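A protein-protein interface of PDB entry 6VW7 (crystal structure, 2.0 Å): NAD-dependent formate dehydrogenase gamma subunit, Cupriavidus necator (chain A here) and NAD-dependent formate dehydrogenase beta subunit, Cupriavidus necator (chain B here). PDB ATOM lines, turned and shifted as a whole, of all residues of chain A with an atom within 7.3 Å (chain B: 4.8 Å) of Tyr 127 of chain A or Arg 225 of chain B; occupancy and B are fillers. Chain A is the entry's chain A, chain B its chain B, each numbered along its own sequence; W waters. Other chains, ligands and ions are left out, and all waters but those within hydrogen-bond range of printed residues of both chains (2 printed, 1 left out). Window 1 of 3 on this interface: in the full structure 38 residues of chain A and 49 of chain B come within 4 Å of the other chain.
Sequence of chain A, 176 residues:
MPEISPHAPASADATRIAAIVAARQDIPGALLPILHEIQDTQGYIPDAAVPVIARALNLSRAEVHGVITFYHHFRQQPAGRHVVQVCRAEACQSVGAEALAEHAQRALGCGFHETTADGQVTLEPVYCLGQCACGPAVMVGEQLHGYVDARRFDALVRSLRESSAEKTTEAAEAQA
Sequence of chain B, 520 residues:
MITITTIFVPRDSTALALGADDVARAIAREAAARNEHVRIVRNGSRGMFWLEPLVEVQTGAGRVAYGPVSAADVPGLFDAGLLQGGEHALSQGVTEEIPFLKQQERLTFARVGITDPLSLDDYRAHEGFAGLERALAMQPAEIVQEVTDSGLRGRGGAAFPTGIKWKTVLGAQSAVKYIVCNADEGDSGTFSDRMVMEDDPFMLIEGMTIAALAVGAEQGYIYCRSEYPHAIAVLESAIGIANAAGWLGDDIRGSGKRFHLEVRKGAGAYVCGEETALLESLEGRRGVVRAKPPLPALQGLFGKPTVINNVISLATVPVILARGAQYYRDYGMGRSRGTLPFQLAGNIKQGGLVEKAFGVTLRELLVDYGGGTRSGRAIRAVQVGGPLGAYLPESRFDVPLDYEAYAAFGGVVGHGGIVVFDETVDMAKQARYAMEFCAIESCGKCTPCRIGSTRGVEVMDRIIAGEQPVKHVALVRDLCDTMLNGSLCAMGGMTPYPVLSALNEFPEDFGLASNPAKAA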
ATOM      1  N   HIS A  72     -21.287  18.692   8.498  1.00  0.00           N
ATOM      2  CA  HIS A  72     -20.856  19.215   7.205  1.00  0.00           C
ATOM      3  C   HIS A  72     -21.269  18.325   6.040  1.00  0.00           C
ATOM      4  O   HIS A  72     -21.353  18.804   4.906  1.00  0.00           O
ATOM      5  CB  HIS A  72     -19.331  19.386   7.204  1.00  0.00           C
ATOM      6  CG  HIS A  72     -18.830  20.388   8.203  1.00  0.00           C
ATOM      7  ND1 HIS A  72     -17.781  20.124   9.060  1.00  0.00           N
ATOM      8  CD2 HIS A  72     -19.220  21.657   8.468  1.00  0.00           C
ATOM      9  CE1 HIS A  72     -17.555  21.184   9.818  1.00  0.00           C
ATOM     10  NE2 HIS A  72     -18.412  22.129   9.476  1.00  0.00           N
ATOM     11  N   GLN A  85     -14.527  16.230  -4.117  1.00  0.00           N
ATOM     12  CA  GLN A  85     -13.912  16.463  -2.809  1.00  0.00           C
ATOM     13  C   GLN A  85     -12.401  16.352  -2.934  1.00  0.00           C
ATOM     14  O   GLN A  85     -11.892  15.322  -3.390  1.00  0.00           O
ATOM     15  CB  GLN A  85     -14.411  15.465  -1.760  1.00  0.00           C
ATOM     16  CG  GLN A  85     -15.918  15.462  -1.571  1.00  0.00           C
ATOM     17  CD  GLN A  85     -16.367  14.362  -0.630  1.00  0.00           C
ATOM     18  OE1 GLN A  85     -16.123  14.434   0.563  1.00  0.00           O
ATOM     19  NE2 GLN A  85     -17.033  13.349  -1.162  1.00  0.00           N
ATOM     20  N   VAL A  86     -11.693  17.400  -2.520  1.00  0.00           N
ATOM     21  CA  VAL A  86     -10.233  17.446  -2.519  1.00  0.00           C
ATOM     22  C   VAL A  86      -9.756  17.359  -1.070  1.00  0.00           C
ATOM     23  O   VAL A  86     -10.125  18.194  -0.232  1.00  0.00           O
ATOM     24  CB  VAL A  86      -9.716  18.727  -3.194  1.00  0.00           C
ATOM     25  CG1 VAL A  86      -8.178  18.784  -3.167  1.00  0.00           C
ATOM     26  CG2 VAL A  86     -10.273  18.838  -4.619  1.00  0.00           C
ATOM     27  N   CYS A  87      -8.930  16.360  -0.773  1.00  0.00           N
ATOM     28  CA  CYS A  87      -8.442  16.206   0.590  1.00  0.00           C
ATOM     29  C   CYS A  87      -7.476  17.328   0.947  1.00  0.00           C
ATOM     30  O   CYS A  87      -6.584  17.666   0.165  1.00  0.00           O
ATOM     31  CB  CYS A  87      -7.761  14.857   0.789  1.00  0.00           C
ATOM     32  SG  CYS A  87      -7.211  14.700   2.514  1.00  0.00           S
ATOM     33  N   ARG A  88      -7.683  17.916   2.127  1.00  0.00           N
ATOM     34  CA  ARG A  88      -6.891  19.028   2.626  1.00  0.00           C
ATOM     35  C   ARG A  88      -6.075  18.673   3.860  1.00  0.00           C
ATOM     36  O   ARG A  88      -5.430  19.556   4.435  1.00  0.00           O
ATOM     37  CB  ARG A  88      -7.800  20.219   2.943  1.00  0.00           C
ATOM     38  CG  ARG A  88      -8.423  20.927   1.737  1.00  0.00           C
ATOM     39  CD  ARG A  88      -8.930  22.287   2.215  1.00  0.00           C
ATOM     40  NE  ARG A  88      -7.873  23.010   2.928  1.00  0.00           N
ATOM     41  CZ  ARG A  88      -8.068  23.742   4.029  1.00  0.00           C
ATOM     42  NH1 ARG A  88      -9.286  23.871   4.551  1.00  0.00           N
ATOM     43  NH2 ARG A  88      -7.039  24.351   4.610  1.00  0.00           N
ATOM     44  N   ALA A  89      -6.103  17.418   4.295  1.00  0.00           N
ATOM     45  CA  ALA A  89      -5.508  17.021   5.562  1.00  0.00           C
ATOM     46  C   ALA A  89      -4.018  16.700   5.392  1.00  0.00           C
ATOM     47  O   ALA A  89      -3.465  16.745   4.288  1.00  0.00           O
ATOM     48  CB  ALA A  89      -6.270  15.837   6.154  1.00  0.00           C
ATOM     49  N   GLU A  90      -3.378  16.317   6.507  1.00  0.00           N
ATOM     50  CA  GLU A  90      -1.922  16.388   6.621  1.00  0.00           C
ATOM     51  C   GLU A  90      -1.190  15.496   5.615  1.00  0.00           C
ATOM     52  O   GLU A  90      -0.211  15.929   5.001  1.00  0.00           O
ATOM     53  CB  GLU A  90      -1.495  16.027   8.046  1.00  0.00           C
ATOM     54  CG  GLU A  90      -1.760  17.129   9.082  1.00  0.00           C
ATOM     55  CD  GLU A  90      -3.166  17.041   9.677  1.00  0.00           C
ATOM     56  OE1 GLU A  90      -4.045  16.383   9.061  1.00  0.00           O
ATOM     57  OE2 GLU A  90      -3.397  17.646  10.751  1.00  0.00           O
ATOM     58  N   GLN A  93      -1.383  16.937   2.306  1.00  0.00           N
ATOM     59  CA  GLN A  93      -0.575  18.157   2.331  1.00  0.00           C
ATOM     60  C   GLN A  93       0.886  17.865   2.051  1.00  0.00           C
ATOM     61  O   GLN A  93       1.558  18.634   1.349  1.00  0.00           O
ATOM     62  CB  GLN A  93      -0.672  18.855   3.686  1.00  0.00           C
ATOM     63  CG  GLN A  93      -1.948  19.597   3.965  1.00  0.00           C
ATOM     64  CD  GLN A  93      -2.029  20.003   5.419  1.00  0.00           C
ATOM     65  OE1 GLN A  93      -0.996  20.164   6.094  1.00  0.00           O
ATOM     66  NE2 GLN A  93      -3.246  20.118   5.931  1.00  0.00           N
ATOM     67  N   PHE A 112     -13.858  26.775  -2.649  1.00  0.00           N
ATOM     68  CA  PHE A 112     -14.432  25.660  -1.914  1.00  0.00           C
ATOM     69  C   PHE A 112     -15.843  26.003  -1.450  1.00  0.00           C
ATOM     70  O   PHE A 112     -16.184  27.169  -1.232  1.00  0.00           O
ATOM     71  CB  PHE A 112     -13.560  25.297  -0.709  1.00  0.00           C
ATOM     72  CG  PHE A 112     -12.386  24.430  -1.051  1.00  0.00           C
ATOM     73  CD1 PHE A 112     -12.562  23.085  -1.341  1.00  0.00           C
ATOM     74  CD2 PHE A 112     -11.106  24.954  -1.081  1.00  0.00           C
ATOM     75  CE1 PHE A 112     -11.484  22.279  -1.659  1.00  0.00           C
ATOM     76  CE2 PHE A 112     -10.024  24.154  -1.392  1.00  0.00           C
ATOM     77  CZ  PHE A 112     -10.214  22.813  -1.682  1.00  0.00           C
ATOM     78  N   HIS A 113     -16.670  24.967  -1.327  1.00  0.00           N
ATOM     79  CA  HIS A 113     -18.085  25.098  -0.993  1.00  0.00           C
ATOM     80  C   HIS A 113     -18.863  25.858  -2.068  1.00  0.00           C
ATOM     81  O   HIS A 113     -19.971  26.336  -1.813  1.00  0.00           O
ATOM     82  CB  HIS A 113     -18.288  25.768   0.375  1.00  0.00           C
ATOM     83  CG  HIS A 113     -17.462  25.172   1.474  1.00  0.00           C
ATOM     84  ND1 HIS A 113     -17.652  23.889   1.941  1.00  0.00           N
ATOM     85  CD2 HIS A 113     -16.448  25.692   2.206  1.00  0.00           C
ATOM     86  CE1 HIS A 113     -16.785  23.642   2.908  1.00  0.00           C
ATOM     87  NE2 HIS A 113     -16.044  24.720   3.088  1.00  0.00           N
ATOM     88  N   PRO A 125     -14.003  20.650   0.252  1.00  0.00           N
ATOM     89  CA  PRO A 125     -12.874  20.046   0.953  1.00  0.00           C
ATOM     90  C   PRO A 125     -13.338  18.803   1.694  1.00  0.00           C
ATOM     91  O   PRO A 125     -14.508  18.658   2.056  1.00  0.00           O
ATOM     92  CB  PRO A 125     -12.426  21.150   1.921  1.00  0.00           C
ATOM     93  CG  PRO A 125     -13.720  21.826   2.293  1.00  0.00           C
ATOM     94  CD  PRO A 125     -14.653  21.690   1.072  1.00  0.00           C
ATOM     95  N   VAL A 126     -12.411  17.878   1.876  1.00  0.00           N
ATOM     96  CA  VAL A 126     -12.606  16.733   2.753  1.00  0.00           C
ATOM     97  C   VAL A 126     -11.330  16.587   3.568  1.00  0.00           C
ATOM     98  O   VAL A 126     -10.249  16.990   3.126  1.00  0.00           O
ATOM     99  CB  VAL A 126     -12.938  15.448   1.955  1.00  0.00           C
ATOM    100  CG1 VAL A 126     -11.802  15.090   0.998  1.00  0.00           C
ATOM    101  CG2 VAL A 126     -13.282  14.281   2.889  1.00  0.00           C
ATOM    102  N   TYR A 127     -11.462  16.059   4.784  1.00  0.00           N
ATOM    103  CA  TYR A 127     -10.342  15.958   5.721  1.00  0.00           C
ATOM    104  C   TYR A 127     -10.024  14.480   5.941  1.00  0.00           C
ATOM    105  O   TYR A 127     -10.493  13.845   6.890  1.00  0.00           O
ATOM    106  CB  TYR A 127     -10.675  16.731   7.021  1.00  0.00           C
ATOM    107  CG  TYR A 127     -10.856  18.199   6.673  1.00  0.00           C
ATOM    108  CD1 TYR A 127      -9.754  19.020   6.458  1.00  0.00           C
ATOM    109  CD2 TYR A 127     -12.123  18.736   6.463  1.00  0.00           C
ATOM    110  CE1 TYR A 127      -9.911  20.353   6.078  1.00  0.00           C
ATOM    111  CE2 TYR A 127     -12.290  20.069   6.100  1.00  0.00           C
ATOM    112  CZ  TYR A 127     -11.190  20.865   5.904  1.00  0.00           C
ATOM    113  OH  TYR A 127     -11.372  22.183   5.531  1.00  0.00           O
ATOM    114  N   CYS A 128      -9.227  13.940   5.012  1.00  0.00           N
ATOM    115  CA  CYS A 128      -8.753  12.557   4.927  1.00  0.00           C
ATOM    116  C   CYS A 128      -9.803  11.607   4.348  1.00  0.00           C
ATOM    117  O   CYS A 128     -10.932  11.504   4.841  1.00  0.00           O
ATOM    118  CB  CYS A 128      -8.272  12.048   6.289  1.00  0.00           C
ATOM    119  SG  CYS A 128      -7.441  10.470   6.181  1.00  0.00           S
ATOM    120  N   LEU A 129      -9.417  10.902   3.290  1.00  0.00           N
ATOM    121  CA  LEU A 129     -10.233   9.853   2.695  1.00  0.00           C
ATOM    122  C   LEU A 129      -9.722   8.461   3.035  1.00  0.00           C
ATOM    123  O   LEU A 129     -10.163   7.480   2.422  1.00  0.00           O
ATOM    124  CB  LEU A 129     -10.286  10.032   1.180  1.00  0.00           C
ATOM    125  CG  LEU A 129     -11.006  11.312   0.742  1.00  0.00           C
ATOM    126  CD1 LEU A 129     -10.640  11.713  -0.701  1.00  0.00           C
ATOM    127  CD2 LEU A 129     -12.510  11.107   0.889  1.00  0.00           C
ATOM    128  N   GLY A 130      -8.798   8.351   3.997  1.00  0.00           N
ATOM    129  CA  GLY A 130      -8.168   7.074   4.254  1.00  0.00           C
ATOM    130  C   GLY A 130      -7.328   6.585   3.094  1.00  0.00           C
ATOM    131  O   GLY A 130      -7.065   5.389   2.987  1.00  0.00           O
ATOM    132  N   GLN A 131      -6.886   7.498   2.228  1.00  0.00           N
ATOM    133  CA  GLN A 131      -6.015   7.209   1.098  1.00  0.00           C
ATOM    134  C   GLN A 131      -4.630   7.820   1.305  1.00  0.00           C
ATOM    135  O   GLN A 131      -3.974   8.225   0.343  1.00  0.00           O
ATOM    136  CB  GLN A 131      -6.633   7.745  -0.193  1.00  0.00           C
ATOM    137  CG  GLN A 131      -8.117   7.318  -0.432  1.00  0.00           C
ATOM    138  CD  GLN A 131      -8.309   5.837  -0.309  1.00  0.00           C
ATOM    139  OE1 GLN A 131      -7.530   5.057  -0.849  1.00  0.00           O
ATOM    140  NE2 GLN A 131      -9.346   5.428   0.430  1.00  0.00           N
ATOM    141  N   ALA B 183     -15.667   3.447  14.406  1.00  0.00           N
ATOM    142  CA  ALA B 183     -15.045   3.390  13.091  1.00  0.00           C
ATOM    143  C   ALA B 183     -14.986   4.776  12.468  1.00  0.00           C
ATOM    144  O   ALA B 183     -15.005   4.920  11.245  1.00  0.00           O
ATOM    145  CB  ALA B 183     -15.792   2.420  12.176  1.00  0.00           C
ATOM    146  N   ASP B 184     -14.901   5.813  13.299  1.00  0.00           N
ATOM    147  CA  ASP B 184     -14.878   7.145  12.723  1.00  0.00           C
ATOM    148  C   ASP B 184     -13.551   7.498  12.061  1.00  0.00           C
ATOM    149  O   ASP B 184     -13.496   8.525  11.379  1.00  0.00           O
ATOM    150  CB  ASP B 184     -15.209   8.188  13.777  1.00  0.00           C
ATOM    151  CG  ASP B 184     -15.731   9.459  13.160  1.00  0.00           C
ATOM    152  OD1 ASP B 184     -16.899   9.451  12.696  1.00  0.00           O
ATOM    153  OD2 ASP B 184     -14.977  10.452  13.097  1.00  0.00           O
ATOM    154  N   GLU B 185     -12.507   6.682  12.243  1.00  0.00           N
ATOM    155  CA  GLU B 185     -11.126   6.923  11.804  1.00  0.00           C
ATOM    156  C   GLU B 185     -10.885   8.256  11.087  1.00  0.00           C
ATOM    157  O   GLU B 185     -10.503   8.280   9.914  1.00  0.00           O
ATOM    158  CB  GLU B 185     -10.671   5.772  10.899  1.00  0.00           C
ATOM    159  CG  GLU B 185      -9.148   5.590  10.861  1.00  0.00           C
ATOM    160  CD  GLU B 185      -8.715   4.361  10.082  1.00  0.00           C
ATOM    161  OE1 GLU B 185      -9.220   4.139   8.951  1.00  0.00           O
ATOM    162  OE2 GLU B 185      -7.875   3.605  10.622  1.00  0.00           O
ATOM    163  N   GLY B 186     -11.107   9.371  11.781  1.00  0.00           N
ATOM    164  CA  GLY B 186     -10.956  10.695  11.190  1.00  0.00           C
ATOM    165  C   GLY B 186      -9.537  11.222  11.065  1.00  0.00           C
ATOM    166  O   GLY B 186      -9.353  12.289  10.473  1.00  0.00           O
ATOM    167  N   TYR B 223     -20.157   2.646  13.943  1.00  0.00           N
ATOM    168  CA  TYR B 223     -20.294   4.043  13.537  1.00  0.00           C
ATOM    169  C   TYR B 223     -19.124   4.356  12.612  1.00  0.00           C
ATOM    170  O   TYR B 223     -17.990   4.529  13.070  1.00  0.00           O
ATOM    171  CB  TYR B 223     -20.339   4.960  14.759  1.00  0.00           C
ATOM    172  CG  TYR B 223     -20.597   6.417  14.434  1.00  0.00           C
ATOM    173  CD1 TYR B 223     -19.551   7.281  14.112  1.00  0.00           C
ATOM    174  CD2 TYR B 223     -21.895   6.931  14.445  1.00  0.00           C
ATOM    175  CE1 TYR B 223     -19.796   8.622  13.802  1.00  0.00           C
ATOM    176  CE2 TYR B 223     -22.148   8.263  14.140  1.00  0.00           C
ATOM    177  CZ  TYR B 223     -21.089   9.111  13.829  1.00  0.00           C
ATOM    178  OH  TYR B 223     -21.333  10.452  13.544  1.00  0.00           O
ATOM    179  N   CYS B 224     -19.396   4.416  11.309  1.00  0.00           N
ATOM    180  CA  CYS B 224     -18.360   4.578  10.295  1.00  0.00           C
ATOM    181  C   CYS B 224     -18.465   5.965   9.665  1.00  0.00           C
ATOM    182  O   CYS B 224     -19.554   6.383   9.271  1.00  0.00           O
ATOM    183  CB  CYS B 224     -18.493   3.489   9.214  1.00  0.00           C
ATOM    184  SG  CYS B 224     -17.174   3.576   8.010  1.00  0.00           S
ATOM    185  N   ARG B 225     -17.334   6.661   9.531  1.00  0.00           N
ATOM    186  CA  ARG B 225     -17.348   8.018   8.980  1.00  0.00           C
ATOM    187  C   ARG B 225     -17.909   8.020   7.557  1.00  0.00           C
ATOM    188  O   ARG B 225     -17.717   7.072   6.793  1.00  0.00           O
ATOM    189  CB  ARG B 225     -15.929   8.607   8.991  1.00  0.00           C
ATOM    190  CG  ARG B 225     -14.917   7.811   8.141  1.00  0.00           C
ATOM    191  CD  ARG B 225     -13.421   8.171   8.499  1.00  0.00           C
ATOM    192  NE  ARG B 225     -13.214   9.618   8.529  1.00  0.00           N
ATOM    193  CZ  ARG B 225     -12.485  10.310   7.654  1.00  0.00           C
ATOM    194  NH1 ARG B 225     -11.848   9.694   6.663  1.00  0.00           N
ATOM    195  NH2 ARG B 225     -12.394  11.627   7.768  1.00  0.00           N
ATOM    196  N   SER B 226     -18.596   9.114   7.196  1.00  0.00           N
ATOM    197  CA  SER B 226     -19.193   9.232   5.864  1.00  0.00           C
ATOM    198  C   SER B 226     -18.149   9.300   4.755  1.00  0.00           C
ATOM    199  O   SER B 226     -18.488   9.082   3.588  1.00  0.00           O
ATOM    200  CB  SER B 226     -20.100  10.474   5.789  1.00  0.00           C
ATOM    201  OG  SER B 226     -19.387  11.638   6.212  1.00  0.00           O
ATOM    202  N   GLU B 227     -16.900   9.634   5.088  1.00  0.00           N
ATOM    203  CA  GLU B 227     -15.812   9.664   4.120  1.00  0.00           C
ATOM    204  C   GLU B 227     -15.405   8.282   3.633  1.00  0.00           C
ATOM    205  O   GLU B 227     -14.572   8.191   2.722  1.00  0.00           O
ATOM    206  CB  GLU B 227     -14.579  10.342   4.758  1.00  0.00           C
ATOM    207  CG  GLU B 227     -14.743  11.833   5.012  1.00  0.00           C
ATOM    208  CD  GLU B 227     -15.461  12.170   6.328  1.00  0.00           C
ATOM    209  OE1 GLU B 227     -15.884  11.268   7.081  1.00  0.00           O
ATOM    210  OE2 GLU B 227     -15.592  13.369   6.616  1.00  0.00           O
ATOM    211  N   TYR B 228     -15.917   7.214   4.255  1.00  0.00           N
ATOM    212  CA  TYR B 228     -15.592   5.837   3.901  1.00  0.00           C
ATOM    213  C   TYR B 228     -16.789   5.114   3.259  1.00  0.00           C
ATOM    214  O   TYR B 228     -17.294   4.145   3.832  1.00  0.00           O
ATOM    215  CB  TYR B 228     -15.172   5.055   5.135  1.00  0.00           C
ATOM    216  CG  TYR B 228     -13.755   5.322   5.687  1.00  0.00           C
ATOM    217  CD1 TYR B 228     -12.852   6.163   5.035  1.00  0.00           C
ATOM    218  CD2 TYR B 228     -13.346   4.707   6.862  1.00  0.00           C
ATOM    219  CE1 TYR B 228     -11.541   6.368   5.554  1.00  0.00           C
ATOM    220  CE2 TYR B 228     -12.055   4.902   7.386  1.00  0.00           C
ATOM    221  CZ  TYR B 228     -11.170   5.727   6.731  1.00  0.00           C
ATOM    222  OH  TYR B 228      -9.916   5.872   7.270  1.00  0.00           O
ATOM    223  N   ILE B 232     -18.493   1.188   4.429  1.00  0.00           N
ATOM    224  CA  ILE B 232     -19.887   1.029   4.814  1.00  0.00           C
ATOM    225  C   ILE B 232     -20.574  -0.011   3.927  1.00  0.00           C
ATOM    226  O   ILE B 232     -21.294  -0.895   4.415  1.00  0.00           O
ATOM    227  CB  ILE B 232     -20.611   2.387   4.753  1.00  0.00           C
ATOM    228  CG1 ILE B 232     -20.105   3.302   5.872  1.00  0.00           C
ATOM    229  CG2 ILE B 232     -22.154   2.165   4.803  1.00  0.00           C
ATOM    230  CD1 ILE B 232     -20.399   4.760   5.638  1.00  0.00           C
ATOM    231  N   GLY B 266     -21.611   8.176   9.683  1.00  0.00           N
ATOM    232  CA  GLY B 266     -21.368   9.483  10.267  1.00  0.00           C
ATOM    233  C   GLY B 266     -21.690  10.580   9.259  1.00  0.00           C
ATOM    234  O   GLY B 266     -22.233  10.331   8.185  1.00  0.00           O
ATOM    235  N   TYR B 433      -2.369  25.349  10.109  1.00  0.00           N
ATOM    236  CA  TYR B 433      -3.378  24.357   9.741  1.00  0.00           C
ATOM    237  C   TYR B 433      -3.957  23.665  10.967  1.00  0.00           C
ATOM    238  O   TYR B 433      -5.169  23.414  11.030  1.00  0.00           O
ATOM    239  CB  TYR B 433      -2.810  23.298   8.794  1.00  0.00           C
ATOM    240  CG  TYR B 433      -3.831  22.194   8.554  1.00  0.00           C
ATOM    241  CD1 TYR B 433      -4.888  22.385   7.677  1.00  0.00           C
ATOM    242  CD2 TYR B 433      -3.757  20.984   9.241  1.00  0.00           C
ATOM    243  CE1 TYR B 433      -5.845  21.383   7.456  1.00  0.00           C
ATOM    244  CE2 TYR B 433      -4.707  19.987   9.043  1.00  0.00           C
ATOM    245  CZ  TYR B 433      -5.747  20.194   8.146  1.00  0.00           C
ATOM    246  OH  TYR B 433      -6.680  19.204   7.948  1.00  0.00           O
ATOM    247  N   PHE B 437      -7.811  23.564  11.498  1.00  0.00           N
ATOM    248  CA  PHE B 437      -8.548  22.311  11.599  1.00  0.00           C
ATOM    249  C   PHE B 437      -9.366  22.258  12.882  1.00  0.00           C
ATOM    250  O   PHE B 437     -10.506  21.776  12.883  1.00  0.00           O
ATOM    251  CB  PHE B 437      -7.577  21.136  11.527  1.00  0.00           C
ATOM    252  CG  PHE B 437      -8.237  19.793  11.566  1.00  0.00           C
ATOM    253  CD1 PHE B 437      -9.078  19.375  10.530  1.00  0.00           C
ATOM    254  CD2 PHE B 437      -8.015  18.937  12.634  1.00  0.00           C
ATOM    255  CE1 PHE B 437      -9.677  18.132  10.569  1.00  0.00           C
ATOM    256  CE2 PHE B 437      -8.611  17.702  12.682  1.00  0.00           C
ATOM    257  CZ  PHE B 437      -9.456  17.294  11.637  1.00  0.00           C
ATOM    258  N   ILE B 440     -12.381  24.404  12.447  1.00  0.00           N
ATOM    259  CA  ILE B 440     -13.363  23.736  11.595  1.00  0.00           C
ATOM    260  C   ILE B 440     -14.111  22.659  12.369  1.00  0.00           C
ATOM    261  O   ILE B 440     -15.337  22.537  12.257  1.00  0.00           O
ATOM    262  CB  ILE B 440     -12.672  23.161  10.345  1.00  0.00           C
ATOM    263  CG1 ILE B 440     -12.231  24.299   9.428  1.00  0.00           C
ATOM    264  CG2 ILE B 440     -13.604  22.185   9.588  1.00  0.00           C
ATOM    265  CD1 ILE B 440     -11.348  23.857   8.299  1.00  0.00           C
ATOM    266  N   GLU B 441     -13.397  21.847  13.150  1.00  0.00           N
ATOM    267  CA  GLU B 441     -14.009  20.659  13.732  1.00  0.00           C
ATOM    268  C   GLU B 441     -14.552  20.861  15.138  1.00  0.00           C
ATOM    269  O   GLU B 441     -15.189  19.948  15.666  1.00  0.00           O
ATOM    270  CB  GLU B 441     -13.018  19.495  13.741  1.00  0.00           C
ATOM    271  CG  GLU B 441     -12.485  19.143  12.361  1.00  0.00           C
ATOM    272  CD  GLU B 441     -13.572  18.573  11.431  1.00  0.00           C
ATOM    273  OE1 GLU B 441     -14.692  18.262  11.897  1.00  0.00           O
ATOM    274  OE2 GLU B 441     -13.298  18.448  10.226  1.00  0.00           O
HETATM  275  O   HOH W   1     -15.597  19.050   8.591  1.00  0.00           O
HETATM  276  O   HOH W   2     -10.820  14.281   9.526  1.00  0.00           O
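The backbone carbonyl oxygen of Tyr 127 of chain A is in hydrogen-bond range of the guanidinium group of Arg 225 of chain B, 3.1 Å away. The backbone carbonyl oxygen (O) of Cys 128 of chain A is in hydrogen-bond range of the guanidinium group (NH1) of Arg 225 of chain B (2.7 Å).
The backbone carbonyl oxygen of Val 86 of chain A is in hydrogen-bond range of the backbone NH of Val 126 of chain A (3.1 Å). The side-chain amide nitrogen of Gln 93 of chain A sits at hydrogen-bond distance from the backbone carbonyl oxygen of Arg 88 of chain A, at 2.7 Å. N of Arg 88 of chain A lies within hydrogen-bond range of O of Val 126 of chain A (2.9 Å). The side-chain hydroxyl (OH) of Tyr 127 of chain A lies within hydrogen-bond range of the guanidinium group (NH1) of Arg 88 of chain A (2.9 Å). O of Asp 184 of chain B lies close to NE of Arg 225 of chain B, at 3.1 Å. NE of Arg 225 of chain B sits close to O of Glu 185 of chain B, 3.3 Å away.
Among the printed residues, merely in contact across the chains: Glu 90 of chain A with Tyr 433 of chain B (3.2 Å), Tyr 127 of chain A with Ile 440 of chain B (3.2 Å), Gln 93 of chain A with Tyr 433 of chain B (3.3 Å), Tyr 127 of chain A with Tyr 433 of chain B (3.4 Å), Ala 89 of chain A with Tyr 433 of chain B (3.4 Å), Val 126 of chain A with Glu 227 of chain B (3.6 Å), Arg 88 of chain A with Tyr 433 of chain B (3.6 Å), His 72 of chain A with Ile 440 of chain B (3.6 Å), Leu 129 of chain A with Tyr 228 of chain B (3.6 Å), Gly 130 of chain A with Tyr 228 of chain B (3.7 Å), Cys 128 of chain A with Glu 227 of chain B (3.8 Å), Tyr 127 of chain A with Phe 437 of chain B (3.9 Å) and Tyr 127 of chain A with Glu 441 of chain B (3.95 Å).
Hydrophobic or aromatic side chains of chain B that line the printed part of chain A: Tyr 228, Tyr 433, Phe 437 and Ile 440. Of the 17 printed residues of chain A, 10 touch a printed residue of chain B. Printed residues of chain A that touch a printed residue of chain B: His 72, Arg 88, Ala 89, Glu 90, Gln 93, Val 126, Tyr 127, Cys 128, Leu 129 and Gly 130. Hydrophobic or aromatic side chains of chain A within 4 Å of the printed part of chain B: His 72, Ala 89, Val 126 and Tyr 127. Among the printed residues, 15 pairs touch across the chains.
Water W1 bridges a ring nitrogen (ND1) of His 72 of chain A (2.5 Å) and the side-chain carboxylate of Glu 441 of chain B (2.9 Å). Water W2 lies within hydrogen-bond range of O of Gly 186 of chain B (2.6 Å) and O of Tyr 127 of chain A (2.7 Å).
Tyr 127 of chain A touches just these residues of chain B: Arg 225, Tyr 433, Phe 437, Ile 440 and Glu 441. Printed residues of chain A within 4 Å of Arg 225 of chain B: Tyr 127 (3.1 Å) and Cys 128 (2.7 Å). Of the printed residues of chain A, Ile 440 of chain B touches His 72 (3.6 Å) and Tyr 127 (3.2 Å). Printed residues of chain B within 4 Å of Gly 130 of chain A: Tyr 228 (3.7 Å). Cys 224 of chain B touches none of the printed residues of chain A.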
